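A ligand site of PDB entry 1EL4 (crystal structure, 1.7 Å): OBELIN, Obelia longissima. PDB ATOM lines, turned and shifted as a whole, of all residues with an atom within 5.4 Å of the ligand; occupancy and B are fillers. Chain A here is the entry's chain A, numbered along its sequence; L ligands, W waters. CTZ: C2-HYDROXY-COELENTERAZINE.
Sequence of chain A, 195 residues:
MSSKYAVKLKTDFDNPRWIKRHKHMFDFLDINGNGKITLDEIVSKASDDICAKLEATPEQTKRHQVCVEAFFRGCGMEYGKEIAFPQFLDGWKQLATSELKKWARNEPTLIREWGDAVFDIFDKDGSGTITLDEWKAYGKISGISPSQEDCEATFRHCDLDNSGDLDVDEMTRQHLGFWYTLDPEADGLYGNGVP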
ATOM      1  N   HIS A  22     -13.311   9.453  16.128  1.00  0.00           N
ATOM      2  CA  HIS A  22     -12.503  10.403  15.379  1.00  0.00           C
ATOM      3  C   HIS A  22     -11.875  11.478  16.270  1.00  0.00           C
ATOM      4  O   HIS A  22     -10.803  11.984  15.955  1.00  0.00           O
ATOM      5  CB  HIS A  22     -13.345  11.019  14.253  1.00  0.00           C
ATOM      6  CG  HIS A  22     -13.594  10.060  13.128  1.00  0.00           C
ATOM      7  ND1 HIS A  22     -12.577   9.618  12.307  1.00  0.00           N
ATOM      8  CD2 HIS A  22     -14.702   9.378  12.767  1.00  0.00           C
ATOM      9  CE1 HIS A  22     -13.050   8.694  11.496  1.00  0.00           C
ATOM     10  NE2 HIS A  22     -14.339   8.527  11.748  1.00  0.00           N
ATOM     11  N   MET A  25      -8.694  10.081  17.459  1.00  0.00           N
ATOM     12  CA  MET A  25      -7.652  10.126  16.448  1.00  0.00           C
ATOM     13  C   MET A  25      -7.180  11.558  16.216  1.00  0.00           C
ATOM     14  O   MET A  25      -5.985  11.795  16.008  1.00  0.00           O
ATOM     15  CB  MET A  25      -8.158   9.507  15.146  1.00  0.00           C
ATOM     16  CG  MET A  25      -8.465   8.023  15.236  1.00  0.00           C
ATOM     17  SD  MET A  25      -7.043   7.059  15.801  1.00  0.00           S
ATOM     18  CE  MET A  25      -5.908   7.331  14.471  1.00  0.00           C
ATOM     19  N   PHE A  26      -8.094  12.510  16.252  1.00  0.00           N
ATOM     20  CA  PHE A  26      -7.711  13.914  16.048  1.00  0.00           C
ATOM     21  C   PHE A  26      -6.724  14.325  17.138  1.00  0.00           C
ATOM     22  O   PHE A  26      -5.684  14.923  16.849  1.00  0.00           O
ATOM     23  CB  PHE A  26      -8.945  14.823  16.120  1.00  0.00           C
ATOM     24  CG  PHE A  26      -8.630  16.272  15.844  1.00  0.00           C
ATOM     25  CD1 PHE A  26      -8.603  16.760  14.542  1.00  0.00           C
ATOM     26  CD2 PHE A  26      -8.339  17.141  16.894  1.00  0.00           C
ATOM     27  CE1 PHE A  26      -8.284  18.081  14.294  1.00  0.00           C
ATOM     28  CE2 PHE A  26      -8.015  18.471  16.646  1.00  0.00           C
ATOM     29  CZ  PHE A  26      -7.993  18.950  15.344  1.00  0.00           C
ATOM     30  N   PHE A  28      -4.848  12.423  18.808  1.00  0.00           N
ATOM     31  CA  PHE A  28      -3.637  11.640  18.585  1.00  0.00           C
ATOM     32  C   PHE A  28      -2.731  12.343  17.563  1.00  0.00           C
ATOM     33  O   PHE A  28      -1.506  12.356  17.713  1.00  0.00           O
ATOM     34  CB  PHE A  28      -4.060  10.234  18.109  1.00  0.00           C
ATOM     35  CG  PHE A  28      -3.039   9.509  17.277  1.00  0.00           C
ATOM     36  CD1 PHE A  28      -1.836   9.078  17.833  1.00  0.00           C
ATOM     37  CD2 PHE A  28      -3.301   9.233  15.943  1.00  0.00           C
ATOM     38  CE1 PHE A  28      -0.917   8.372  17.063  1.00  0.00           C
ATOM     39  CE2 PHE A  28      -2.382   8.526  15.163  1.00  0.00           C
ATOM     40  CZ  PHE A  28      -1.188   8.100  15.728  1.00  0.00           C
ATOM     41  N   LEU A  29      -3.338  12.950  16.546  1.00  0.00           N
ATOM     42  CA  LEU A  29      -2.584  13.671  15.522  1.00  0.00           C
ATOM     43  C   LEU A  29      -2.188  15.069  15.997  1.00  0.00           C
ATOM     44  O   LEU A  29      -1.200  15.631  15.527  1.00  0.00           O
ATOM     45  CB  LEU A  29      -3.421  13.804  14.243  1.00  0.00           C
ATOM     46  CG  LEU A  29      -3.762  12.499  13.515  1.00  0.00           C
ATOM     47  CD1 LEU A  29      -4.703  12.783  12.339  1.00  0.00           C
ATOM     48  CD2 LEU A  29      -2.475  11.840  13.016  1.00  0.00           C
ATOM     49  N   ILE A  42       0.343  15.760   8.819  1.00  0.00           N
ATOM     50  CA  ILE A  42      -0.081  14.387   8.551  1.00  0.00           C
ATOM     51  C   ILE A  42       0.862  13.724   7.544  1.00  0.00           C
ATOM     52  O   ILE A  42       1.270  12.567   7.725  1.00  0.00           O
ATOM     53  CB  ILE A  42      -1.529  14.348   8.015  1.00  0.00           C
ATOM     54  CG1 ILE A  42      -2.497  14.634   9.165  1.00  0.00           C
ATOM     55  CG2 ILE A  42      -1.831  12.996   7.388  1.00  0.00           C
ATOM     56  CD1 ILE A  42      -3.957  14.649   8.753  1.00  0.00           C
ATOM     57  N   LYS A  45       4.201  13.002   9.072  1.00  0.00           N
ATOM     58  CA  LYS A  45       4.091  11.819   9.922  1.00  0.00           C
ATOM     59  C   LYS A  45       4.181  10.563   9.053  1.00  0.00           C
ATOM     60  O   LYS A  45       4.860   9.602   9.407  1.00  0.00           O
ATOM     61  CB  LYS A  45       2.748  11.828  10.671  1.00  0.00           C
ATOM     62  CG  LYS A  45       2.509  10.607  11.548  1.00  0.00           C
ATOM     63  CD  LYS A  45       1.106  10.660  12.156  1.00  0.00           C
ATOM     64  CE  LYS A  45       0.830   9.437  13.040  1.00  0.00           C
ATOM     65  NZ  LYS A  45       1.732   9.373  14.222  1.00  0.00           N
ATOM     66  N   ALA A  46       3.493  10.589   7.921  1.00  0.00           N
ATOM     67  CA  ALA A  46       3.478   9.448   7.019  1.00  0.00           C
ATOM     68  C   ALA A  46       4.822   9.189   6.335  1.00  0.00           C
ATOM     69  O   ALA A  46       5.301   8.061   6.305  1.00  0.00           O
ATOM     70  CB  ALA A  46       2.388   9.623   5.970  1.00  0.00           C
ATOM     71  N   ILE A  50       6.869   7.558   9.780  1.00  0.00           N
ATOM     72  CA  ILE A  50       6.509   6.164   9.549  1.00  0.00           C
ATOM     73  C   ILE A  50       7.298   5.454   8.457  1.00  0.00           C
ATOM     74  O   ILE A  50       7.949   4.444   8.735  1.00  0.00           O
ATOM     75  CB  ILE A  50       5.009   6.050   9.233  1.00  0.00           C
ATOM     76  CG1 ILE A  50       4.201   6.494  10.453  1.00  0.00           C
ATOM     77  CG2 ILE A  50       4.638   4.603   8.878  1.00  0.00           C
ATOM     78  CD1 ILE A  50       2.702   6.526  10.217  1.00  0.00           C
ATOM     79  N   HIS A  64       2.897   5.841  -1.020  1.00  0.00           N
ATOM     80  CA  HIS A  64       2.176   5.938   0.245  1.00  0.00           C
ATOM     81  C   HIS A  64       1.743   7.386   0.486  1.00  0.00           C
ATOM     82  O   HIS A  64       0.604   7.648   0.889  1.00  0.00           O
ATOM     83  CB  HIS A  64       3.062   5.426   1.388  1.00  0.00           C
ATOM     84  CG  HIS A  64       2.412   5.443   2.730  1.00  0.00           C
ATOM     85  ND1 HIS A  64       2.591   6.467   3.639  1.00  0.00           N
ATOM     86  CD2 HIS A  64       1.582   4.559   3.327  1.00  0.00           C
ATOM     87  CE1 HIS A  64       1.913   6.209   4.744  1.00  0.00           C
ATOM     88  NE2 HIS A  64       1.286   5.058   4.582  1.00  0.00           N
ATOM     89  N   VAL A  68      -2.016   8.972   1.125  1.00  0.00           N
ATOM     90  CA  VAL A  68      -2.341   9.715   2.334  1.00  0.00           C
ATOM     91  C   VAL A  68      -2.884  11.093   1.950  1.00  0.00           C
ATOM     92  O   VAL A  68      -3.866  11.570   2.506  1.00  0.00           O
ATOM     93  CB  VAL A  68      -1.102   9.867   3.234  1.00  0.00           C
ATOM     94  CG1 VAL A  68      -1.391  10.806   4.398  1.00  0.00           C
ATOM     95  CG2 VAL A  68      -0.687   8.487   3.772  1.00  0.00           C
ATOM     96  N   PHE A  72      -6.742  12.264   3.077  1.00  0.00           N
ATOM     97  CA  PHE A  72      -7.077  13.403   3.905  1.00  0.00           C
ATOM     98  C   PHE A  72      -7.579  14.614   3.153  1.00  0.00           C
ATOM     99  O   PHE A  72      -8.210  15.495   3.745  1.00  0.00           O
ATOM    100  CB  PHE A  72      -5.918  13.711   4.849  1.00  0.00           C
ATOM    101  CG  PHE A  72      -5.744  12.676   5.918  1.00  0.00           C
ATOM    102  CD1 PHE A  72      -4.785  11.677   5.790  1.00  0.00           C
ATOM    103  CD2 PHE A  72      -6.608  12.640   7.010  1.00  0.00           C
ATOM    104  CE1 PHE A  72      -4.691  10.652   6.731  1.00  0.00           C
ATOM    105  CE2 PHE A  72      -6.524  11.622   7.960  1.00  0.00           C
ATOM    106  CZ  PHE A  72      -5.564  10.621   7.822  1.00  0.00           C
ATOM    107  N   PHE A  88     -12.835  19.009  10.763  1.00  0.00           N
ATOM    108  CA  PHE A  88     -12.261  17.689  10.533  1.00  0.00           C
ATOM    109  C   PHE A  88     -13.385  16.655  10.504  1.00  0.00           C
ATOM    110  O   PHE A  88     -13.460  15.815   9.596  1.00  0.00           O
ATOM    111  CB  PHE A  88     -11.274  17.372  11.656  1.00  0.00           C
ATOM    112  CG  PHE A  88     -10.513  16.086  11.464  1.00  0.00           C
ATOM    113  CD1 PHE A  88      -9.496  15.979  10.514  1.00  0.00           C
ATOM    114  CD2 PHE A  88     -10.765  14.996  12.301  1.00  0.00           C
ATOM    115  CE1 PHE A  88      -8.735  14.818  10.406  1.00  0.00           C
ATOM    116  CE2 PHE A  88     -10.009  13.827  12.193  1.00  0.00           C
ATOM    117  CZ  PHE A  88      -8.992  13.743  11.250  1.00  0.00           C
ATOM    118  N   TRP A  92     -14.914  14.206   7.542  1.00  0.00           N
ATOM    119  CA  TRP A  92     -15.048  12.759   7.618  1.00  0.00           C
ATOM    120  C   TRP A  92     -16.422  12.304   7.186  1.00  0.00           C
ATOM    121  O   TRP A  92     -16.591  11.209   6.642  1.00  0.00           O
ATOM    122  CB  TRP A  92     -14.747  12.243   9.027  1.00  0.00           C
ATOM    123  CG  TRP A  92     -13.311  11.857   9.197  1.00  0.00           C
ATOM    124  CD1 TRP A  92     -12.290  12.635   9.650  1.00  0.00           C
ATOM    125  CD2 TRP A  92     -12.741  10.586   8.859  1.00  0.00           C
ATOM    126  NE1 TRP A  92     -11.106  11.933   9.616  1.00  0.00           N
ATOM    127  CE2 TRP A  92     -11.355  10.669   9.131  1.00  0.00           C
ATOM    128  CE3 TRP A  92     -13.258   9.393   8.346  1.00  0.00           C
ATOM    129  CZ2 TRP A  92     -10.478   9.604   8.915  1.00  0.00           C
ATOM    130  CZ3 TRP A  92     -12.394   8.325   8.130  1.00  0.00           C
ATOM    131  CH2 TRP A  92     -11.018   8.438   8.418  1.00  0.00           C
ATOM    132  N   ILE A 111      -9.540   4.233   1.086  1.00  0.00           N
ATOM    133  CA  ILE A 111      -8.997   3.477   2.212  1.00  0.00           C
ATOM    134  C   ILE A 111      -8.365   2.187   1.698  1.00  0.00           C
ATOM    135  O   ILE A 111      -7.340   1.740   2.224  1.00  0.00           O
ATOM    136  CB  ILE A 111     -10.089   3.178   3.295  1.00  0.00           C
ATOM    137  CG1 ILE A 111      -9.464   2.440   4.484  1.00  0.00           C
ATOM    138  CG2 ILE A 111     -11.240   2.379   2.695  1.00  0.00           C
ATOM    139  CD1 ILE A 111      -8.438   3.247   5.247  1.00  0.00           C
ATOM    140  N   TRP A 114      -5.005   3.216   0.196  1.00  0.00           N
ATOM    141  CA  TRP A 114      -4.025   3.554   1.215  1.00  0.00           C
ATOM    142  C   TRP A 114      -3.541   2.214   1.751  1.00  0.00           C
ATOM    143  O   TRP A 114      -2.346   2.007   1.961  1.00  0.00           O
ATOM    144  CB  TRP A 114      -4.688   4.391   2.327  1.00  0.00           C
ATOM    145  CG  TRP A 114      -3.755   4.833   3.429  1.00  0.00           C
ATOM    146  CD1 TRP A 114      -2.405   4.639   3.506  1.00  0.00           C
ATOM    147  CD2 TRP A 114      -4.123   5.521   4.643  1.00  0.00           C
ATOM    148  NE1 TRP A 114      -1.908   5.168   4.679  1.00  0.00           N
ATOM    149  CE2 TRP A 114      -2.947   5.706   5.394  1.00  0.00           C
ATOM    150  CE3 TRP A 114      -5.336   5.987   5.155  1.00  0.00           C
ATOM    151  CZ2 TRP A 114      -2.939   6.352   6.639  1.00  0.00           C
ATOM    152  CZ3 TRP A 114      -5.340   6.630   6.399  1.00  0.00           C
ATOM    153  CH2 TRP A 114      -4.146   6.801   7.122  1.00  0.00           C
ATOM    154  N   GLY A 115      -4.474   1.289   1.942  1.00  0.00           N
ATOM    155  CA  GLY A 115      -4.123  -0.037   2.417  1.00  0.00           C
ATOM    156  C   GLY A 115      -3.147  -0.723   1.486  1.00  0.00           C
ATOM    157  O   GLY A 115      -2.179  -1.329   1.950  1.00  0.00           O
ATOM    158  N   VAL A 118       0.308   0.541   2.224  1.00  0.00           N
ATOM    159  CA  VAL A 118       0.860   0.085   3.489  1.00  0.00           C
ATOM    160  C   VAL A 118       1.271  -1.375   3.349  1.00  0.00           C
ATOM    161  O   VAL A 118       2.388  -1.741   3.718  1.00  0.00           O
ATOM    162  CB  VAL A 118      -0.156   0.224   4.637  1.00  0.00           C
ATOM    163  CG1 VAL A 118       0.368  -0.448   5.901  1.00  0.00           C
ATOM    164  CG2 VAL A 118      -0.427   1.697   4.896  1.00  0.00           C
ATOM    165  N   PHE A 119       0.369  -2.206   2.831  1.00  0.00           N
ATOM    166  CA  PHE A 119       0.682  -3.624   2.658  1.00  0.00           C
ATOM    167  C   PHE A 119       1.894  -3.806   1.742  1.00  0.00           C
ATOM    168  O   PHE A 119       2.716  -4.690   1.963  1.00  0.00           O
ATOM    169  CB  PHE A 119      -0.518  -4.381   2.079  1.00  0.00           C
ATOM    170  CG  PHE A 119      -1.528  -4.813   3.116  1.00  0.00           C
ATOM    171  CD1 PHE A 119      -2.315  -3.881   3.781  1.00  0.00           C
ATOM    172  CD2 PHE A 119      -1.679  -6.167   3.430  1.00  0.00           C
ATOM    173  CE1 PHE A 119      -3.237  -4.281   4.739  1.00  0.00           C
ATOM    174  CE2 PHE A 119      -2.606  -6.574   4.398  1.00  0.00           C
ATOM    175  CZ  PHE A 119      -3.388  -5.635   5.052  1.00  0.00           C
ATOM    176  N   TRP A 135       2.432  -6.071  11.695  1.00  0.00           N
ATOM    177  CA  TRP A 135       1.408  -5.138  12.163  1.00  0.00           C
ATOM    178  C   TRP A 135       1.846  -4.512  13.490  1.00  0.00           C
ATOM    179  O   TRP A 135       1.639  -3.324  13.712  1.00  0.00           O
ATOM    180  CB  TRP A 135       0.066  -5.850  12.337  1.00  0.00           C
ATOM    181  CG  TRP A 135      -1.046  -4.909  12.727  1.00  0.00           C
ATOM    182  CD1 TRP A 135      -1.756  -4.899  13.893  1.00  0.00           C
ATOM    183  CD2 TRP A 135      -1.539  -3.810  11.951  1.00  0.00           C
ATOM    184  NE1 TRP A 135      -2.664  -3.861  13.898  1.00  0.00           N
ATOM    185  CE2 TRP A 135      -2.547  -3.180  12.726  1.00  0.00           C
ATOM    186  CE3 TRP A 135      -1.231  -3.284  10.692  1.00  0.00           C
ATOM    187  CZ2 TRP A 135      -3.254  -2.051  12.265  1.00  0.00           C
ATOM    188  CZ3 TRP A 135      -1.921  -2.165  10.234  1.00  0.00           C
ATOM    189  CH2 TRP A 135      -2.922  -1.560  11.023  1.00  0.00           C
ATOM    190  N   TYR A 138       4.046  -1.708  12.761  1.00  0.00           N
ATOM    191  CA  TYR A 138       3.315  -0.545  12.275  1.00  0.00           C
ATOM    192  C   TYR A 138       2.593   0.155  13.423  1.00  0.00           C
ATOM    193  O   TYR A 138       2.642   1.382  13.555  1.00  0.00           O
ATOM    194  CB  TYR A 138       2.286  -0.940  11.220  1.00  0.00           C
ATOM    195  CG  TYR A 138       1.514   0.243  10.697  1.00  0.00           C
ATOM    196  CD1 TYR A 138       2.081   1.106   9.762  1.00  0.00           C
ATOM    197  CD2 TYR A 138       0.249   0.554  11.206  1.00  0.00           C
ATOM    198  CE1 TYR A 138       1.411   2.252   9.342  1.00  0.00           C
ATOM    199  CE2 TYR A 138      -0.421   1.701  10.797  1.00  0.00           C
ATOM    200  CZ  TYR A 138       0.166   2.541   9.866  1.00  0.00           C
ATOM    201  OH  TYR A 138      -0.492   3.696   9.486  1.00  0.00           O
ATOM    202  N   SER A 142       3.551   3.938  13.961  1.00  0.00           N
ATOM    203  CA  SER A 142       2.538   4.934  13.651  1.00  0.00           C
ATOM    204  C   SER A 142       1.954   5.467  14.954  1.00  0.00           C
ATOM    205  O   SER A 142       1.422   6.571  15.015  1.00  0.00           O
ATOM    206  CB  SER A 142       1.410   4.318  12.814  1.00  0.00           C
ATOM    207  OG  SER A 142       0.668   3.389  13.585  1.00  0.00           O
ATOM    208  N   ILE A 144      -0.613   4.301  16.437  1.00  0.00           N
ATOM    209  CA  ILE A 144      -2.055   4.065  16.517  1.00  0.00           C
ATOM    210  C   ILE A 144      -2.389   2.893  17.440  1.00  0.00           C
ATOM    211  O   ILE A 144      -3.451   2.851  18.044  1.00  0.00           O
ATOM    212  CB  ILE A 144      -2.674   3.816  15.124  1.00  0.00           C
ATOM    213  CG1 ILE A 144      -4.204   3.877  15.207  1.00  0.00           C
ATOM    214  CG2 ILE A 144      -2.247   2.445  14.588  1.00  0.00           C
ATOM    215  CD1 ILE A 144      -4.899   3.873  13.855  1.00  0.00           C
ATOM    216  N   VAL A 168      -5.216  -7.447   2.638  1.00  0.00           N
ATOM    217  CA  VAL A 168      -5.841  -6.140   2.461  1.00  0.00           C
ATOM    218  C   VAL A 168      -7.361  -6.164   2.232  1.00  0.00           C
ATOM    219  O   VAL A 168      -8.072  -5.244   2.652  1.00  0.00           O
ATOM    220  CB  VAL A 168      -5.155  -5.368   1.314  1.00  0.00           C
ATOM    221  CG1 VAL A 168      -5.493  -6.007  -0.025  1.00  0.00           C
ATOM    222  CG2 VAL A 168      -5.572  -3.905   1.342  1.00  0.00           C
ATOM    223  N   MET A 171      -8.815  -6.373   5.739  1.00  0.00           N
ATOM    224  CA  MET A 171      -8.575  -5.156   6.503  1.00  0.00           C
ATOM    225  C   MET A 171      -9.382  -3.977   5.968  1.00  0.00           C
ATOM    226  O   MET A 171      -9.859  -3.144   6.749  1.00  0.00           O
ATOM    227  CB  MET A 171      -7.086  -4.811   6.522  1.00  0.00           C
ATOM    228  CG  MET A 171      -6.744  -3.754   7.549  1.00  0.00           C
ATOM    229  SD  MET A 171      -7.273  -4.262   9.205  1.00  0.00           S
ATOM    230  CE  MET A 171      -6.193  -3.273  10.230  1.00  0.00           C
ATOM    231  N   THR A 172      -9.556  -3.909   4.651  1.00  0.00           N
ATOM    232  CA  THR A 172     -10.323  -2.817   4.060  1.00  0.00           C
ATOM    233  C   THR A 172     -11.771  -2.879   4.540  1.00  0.00           C
ATOM    234  O   THR A 172     -12.353  -1.864   4.914  1.00  0.00           O
ATOM    235  CB  THR A 172     -10.285  -2.882   2.524  1.00  0.00           C
ATOM    236  OG1 THR A 172      -8.927  -2.707   2.072  1.00  0.00           O
ATOM    237  CG2 THR A 172     -11.149  -1.782   1.915  1.00  0.00           C
ATOM    238  N   HIS A 175     -11.819  -1.730   8.190  1.00  0.00           N
ATOM    239  CA  HIS A 175     -11.587  -0.287   8.294  1.00  0.00           C
ATOM    240  C   HIS A 175     -12.788   0.527   7.855  1.00  0.00           C
ATOM    241  O   HIS A 175     -13.077   1.578   8.426  1.00  0.00           O
ATOM    242  CB  HIS A 175     -10.365   0.103   7.469  1.00  0.00           C
ATOM    243  CG  HIS A 175      -9.078   0.039   8.232  1.00  0.00           C
ATOM    244  ND1 HIS A 175      -7.848  -0.054   7.618  1.00  0.00           N
ATOM    245  CD2 HIS A 175      -8.842   0.063   9.560  1.00  0.00           C
ATOM    246  CE1 HIS A 175      -6.906  -0.074   8.544  1.00  0.00           C
ATOM    247  NE2 HIS A 175      -7.480  -0.002   9.730  1.00  0.00           N
ATOM    248  N   TRP A 179     -14.088   3.048  10.569  1.00  0.00           N
ATOM    249  CA  TRP A 179     -13.981   4.498  10.370  1.00  0.00           C
ATOM    250  C   TRP A 179     -15.184   5.202   9.755  1.00  0.00           C
ATOM    251  O   TRP A 179     -15.418   6.375  10.028  1.00  0.00           O
ATOM    252  CB  TRP A 179     -12.768   4.817   9.484  1.00  0.00           C
ATOM    253  CG  TRP A 179     -11.449   4.313   9.998  1.00  0.00           C
ATOM    254  CD1 TRP A 179     -10.542   3.563   9.294  1.00  0.00           C
ATOM    255  CD2 TRP A 179     -10.867   4.549  11.278  1.00  0.00           C
ATOM    256  NE1 TRP A 179      -9.440   3.318  10.070  1.00  0.00           N
ATOM    257  CE2 TRP A 179      -9.612   3.904  11.291  1.00  0.00           C
ATOM    258  CE3 TRP A 179     -11.279   5.244  12.427  1.00  0.00           C
ATOM    259  CZ2 TRP A 179      -8.763   3.933  12.406  1.00  0.00           C
ATOM    260  CZ3 TRP A 179     -10.435   5.264  13.533  1.00  0.00           C
ATOM    261  CH2 TRP A 179      -9.187   4.619  13.515  1.00  0.00           C
ATOM    262  N   TYR A 190      -9.220  -2.339  16.860  1.00  0.00           N
ATOM    263  CA  TYR A 190      -7.928  -1.942  17.396  1.00  0.00           C
ATOM    264  C   TYR A 190      -7.789  -2.275  18.879  1.00  0.00           C
ATOM    265  O   TYR A 190      -7.015  -1.640  19.600  1.00  0.00           O
ATOM    266  CB  TYR A 190      -7.687  -0.445  17.179  1.00  0.00           C
ATOM    267  CG  TYR A 190      -7.325  -0.071  15.753  1.00  0.00           C
ATOM    268  CD1 TYR A 190      -8.310   0.192  14.800  1.00  0.00           C
ATOM    269  CD2 TYR A 190      -5.994   0.009  15.354  1.00  0.00           C
ATOM    270  CE1 TYR A 190      -7.976   0.523  13.479  1.00  0.00           C
ATOM    271  CE2 TYR A 190      -5.647   0.345  14.044  1.00  0.00           C
ATOM    272  CZ  TYR A 190      -6.630   0.599  13.122  1.00  0.00           C
ATOM    273  OH  TYR A 190      -6.280   0.925  11.834  1.00  0.00           O
HETATM  274  N1  CTZ L   1      -3.205   3.901   9.834  1.00  0.00           N
HETATM  275  C2  CTZ L   1      -4.011   2.963   9.266  1.00  0.00           C
HETATM  276  C3  CTZ L   1      -5.335   3.381   9.240  1.00  0.00           C
HETATM  277  N4  CTZ L   1      -5.346   4.646   9.849  1.00  0.00           N
HETATM  278  C5  CTZ L   1      -6.420   5.565  10.133  1.00  0.00           C
HETATM  279  C6  CTZ L   1      -6.073   6.778  10.783  1.00  0.00           C
HETATM  280  N7  CTZ L   1      -4.715   7.035  11.120  1.00  0.00           N
HETATM  281  C8  CTZ L   1      -3.659   6.152  10.860  1.00  0.00           C
HETATM  282  C9  CTZ L   1      -3.988   4.953  10.219  1.00  0.00           C
HETATM  283  C10 CTZ L   1      -3.152   2.493   8.074  1.00  0.00           C
HETATM  284  C11 CTZ L   1      -3.709   1.462   7.110  1.00  0.00           C
HETATM  285  C12 CTZ L   1      -3.361   0.089   7.338  1.00  0.00           C
HETATM  286  C13 CTZ L   1      -4.011  -0.977   6.637  1.00  0.00           C
HETATM  287  C14 CTZ L   1      -5.030  -0.669   5.696  1.00  0.00           C
HETATM  288  C15 CTZ L   1      -5.412   0.698   5.435  1.00  0.00           C
HETATM  289  C16 CTZ L   1      -4.754   1.759   6.138  1.00  0.00           C
HETATM  290  O17 CTZ L   1      -5.649  -1.689   5.040  1.00  0.00           O
HETATM  291  O18 CTZ L   1      -6.376   2.910   8.843  1.00  0.00           O
HETATM  292  C19 CTZ L   1      -7.069   7.753  11.146  1.00  0.00           C
HETATM  293  C20 CTZ L   1      -8.440   7.404  11.418  1.00  0.00           C
HETATM  294  C21 CTZ L   1      -9.392   8.379  11.793  1.00  0.00           C
HETATM  295  C22 CTZ L   1      -8.993   9.748  11.899  1.00  0.00           C
HETATM  296  C23 CTZ L   1      -7.643  10.145  11.638  1.00  0.00           C
HETATM  297  C24 CTZ L   1      -6.683   9.142  11.257  1.00  0.00           C
HETATM  298  O25 CTZ L   1      -9.916  10.671  12.273  1.00  0.00           O
HETATM  299  C26 CTZ L   1      -2.334   6.600  11.290  1.00  0.00           C
HETATM  300  C27 CTZ L   1      -1.742   7.635  10.372  1.00  0.00           C
HETATM  301  C28 CTZ L   1      -0.688   7.277   9.460  1.00  0.00           C
HETATM  302  C29 CTZ L   1      -0.110   8.254   8.570  1.00  0.00           C
HETATM  303  C30 CTZ L   1      -0.589   9.601   8.580  1.00  0.00           C
HETATM  304  C31 CTZ L   1      -1.650   9.985   9.477  1.00  0.00           C
HETATM  305  C32 CTZ L   1      -2.220   9.003  10.369  1.00  0.00           C
HETATM  306  O33 CTZ L   1      -3.823   1.699   9.984  1.00  0.00           O
HETATM  307  O   HOH W   1      -7.669  -0.778   3.532  1.00  0.00           O
HETATM  308  O   HOH W   2       0.446   4.929   7.369  1.00  0.00           O
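Merely in contact with the ligand: Phe 88, Met 25, Gly 115, Met 171, Trp 135, Phe 119, Ile 50, Ile 42, Trp 114, Ala 46, Ile 111, Leu 29, Ile 144, Lys 45, Phe 72 and Val 118.
Hydrophobic or aromatic side chains that line the ligand: His 22, Met 25, Leu 29, Ile 42, Ala 46, Ile 50, Phe 72, Phe 88, Trp 92, Ile 111, Trp 114, Val 118, Phe 119, Trp 135, Tyr 138, Ile 144, Met 171, His 175 and Trp 179.
Of the 29 residues printed, 22 come within 4 Å of the ligand.
The nearest printed residue that does not touch the ligand is Val 168 (4.3 Å).
Water W1 lies within hydrogen-bond range of O17 of the ligand, OG1 of Thr 172 and O of Ile 111.
Water W2 lies within hydrogen-bond range of OH of Tyr 138 and NE2 of His 64.
NE1 of Trp 179 lies within hydrogen-bond range of O18 of the ligand.
The indole nitrogen of Trp 92 sits at hydrogen-bond distance from an oxygen (O25) of the ligand, 3.2 Å away.
OH of Tyr 138 lies within hydrogen-bond range of N1 of the ligand, 2.7 Å away.
O33 of the ligand is in hydrogen-bond range of OH of Tyr 190 (3.2 Å).
A ring nitrogen (ND1) of His 22 lies within hydrogen-bond range of an oxygen (O25) of the ligand (2.9 Å).
A ring nitrogen (NE2) of His 175 sits close to an oxygen (O18) of the ligand.
The side-chain hydroxyl (OG) of Ser 142 lies close to the backbone NH (N) of Ile 144 (3.3 Å).
The backbone carbonyl oxygen (O) of Tyr 138 is in hydrogen-bond range of the side-chain hydroxyl (OG) of Ser 142.
A ring nitrogen (NE2) of His 22 is in hydrogen-bond range of the backbone carbonyl oxygen (O) of Trp 179.
The backbone carbonyl oxygen (O) of Ser 142 sits at hydrogen-bond distance from the side-chain amino group (NZ) of Lys 45, 2.9 Å away.
The backbone NH (N) of Ile 50 lies within hydrogen-bond range of the backbone carbonyl oxygen (O) of Lys 45 (2.9 Å).
A ring nitrogen (NE2) of His 175 lies within hydrogen-bond range of the side-chain hydroxyl (OH) of Tyr 190 (2.6 Å).
NE2 of His 64 lies within hydrogen-bond range of NE1 of Trp 114, 3.2 Å away.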
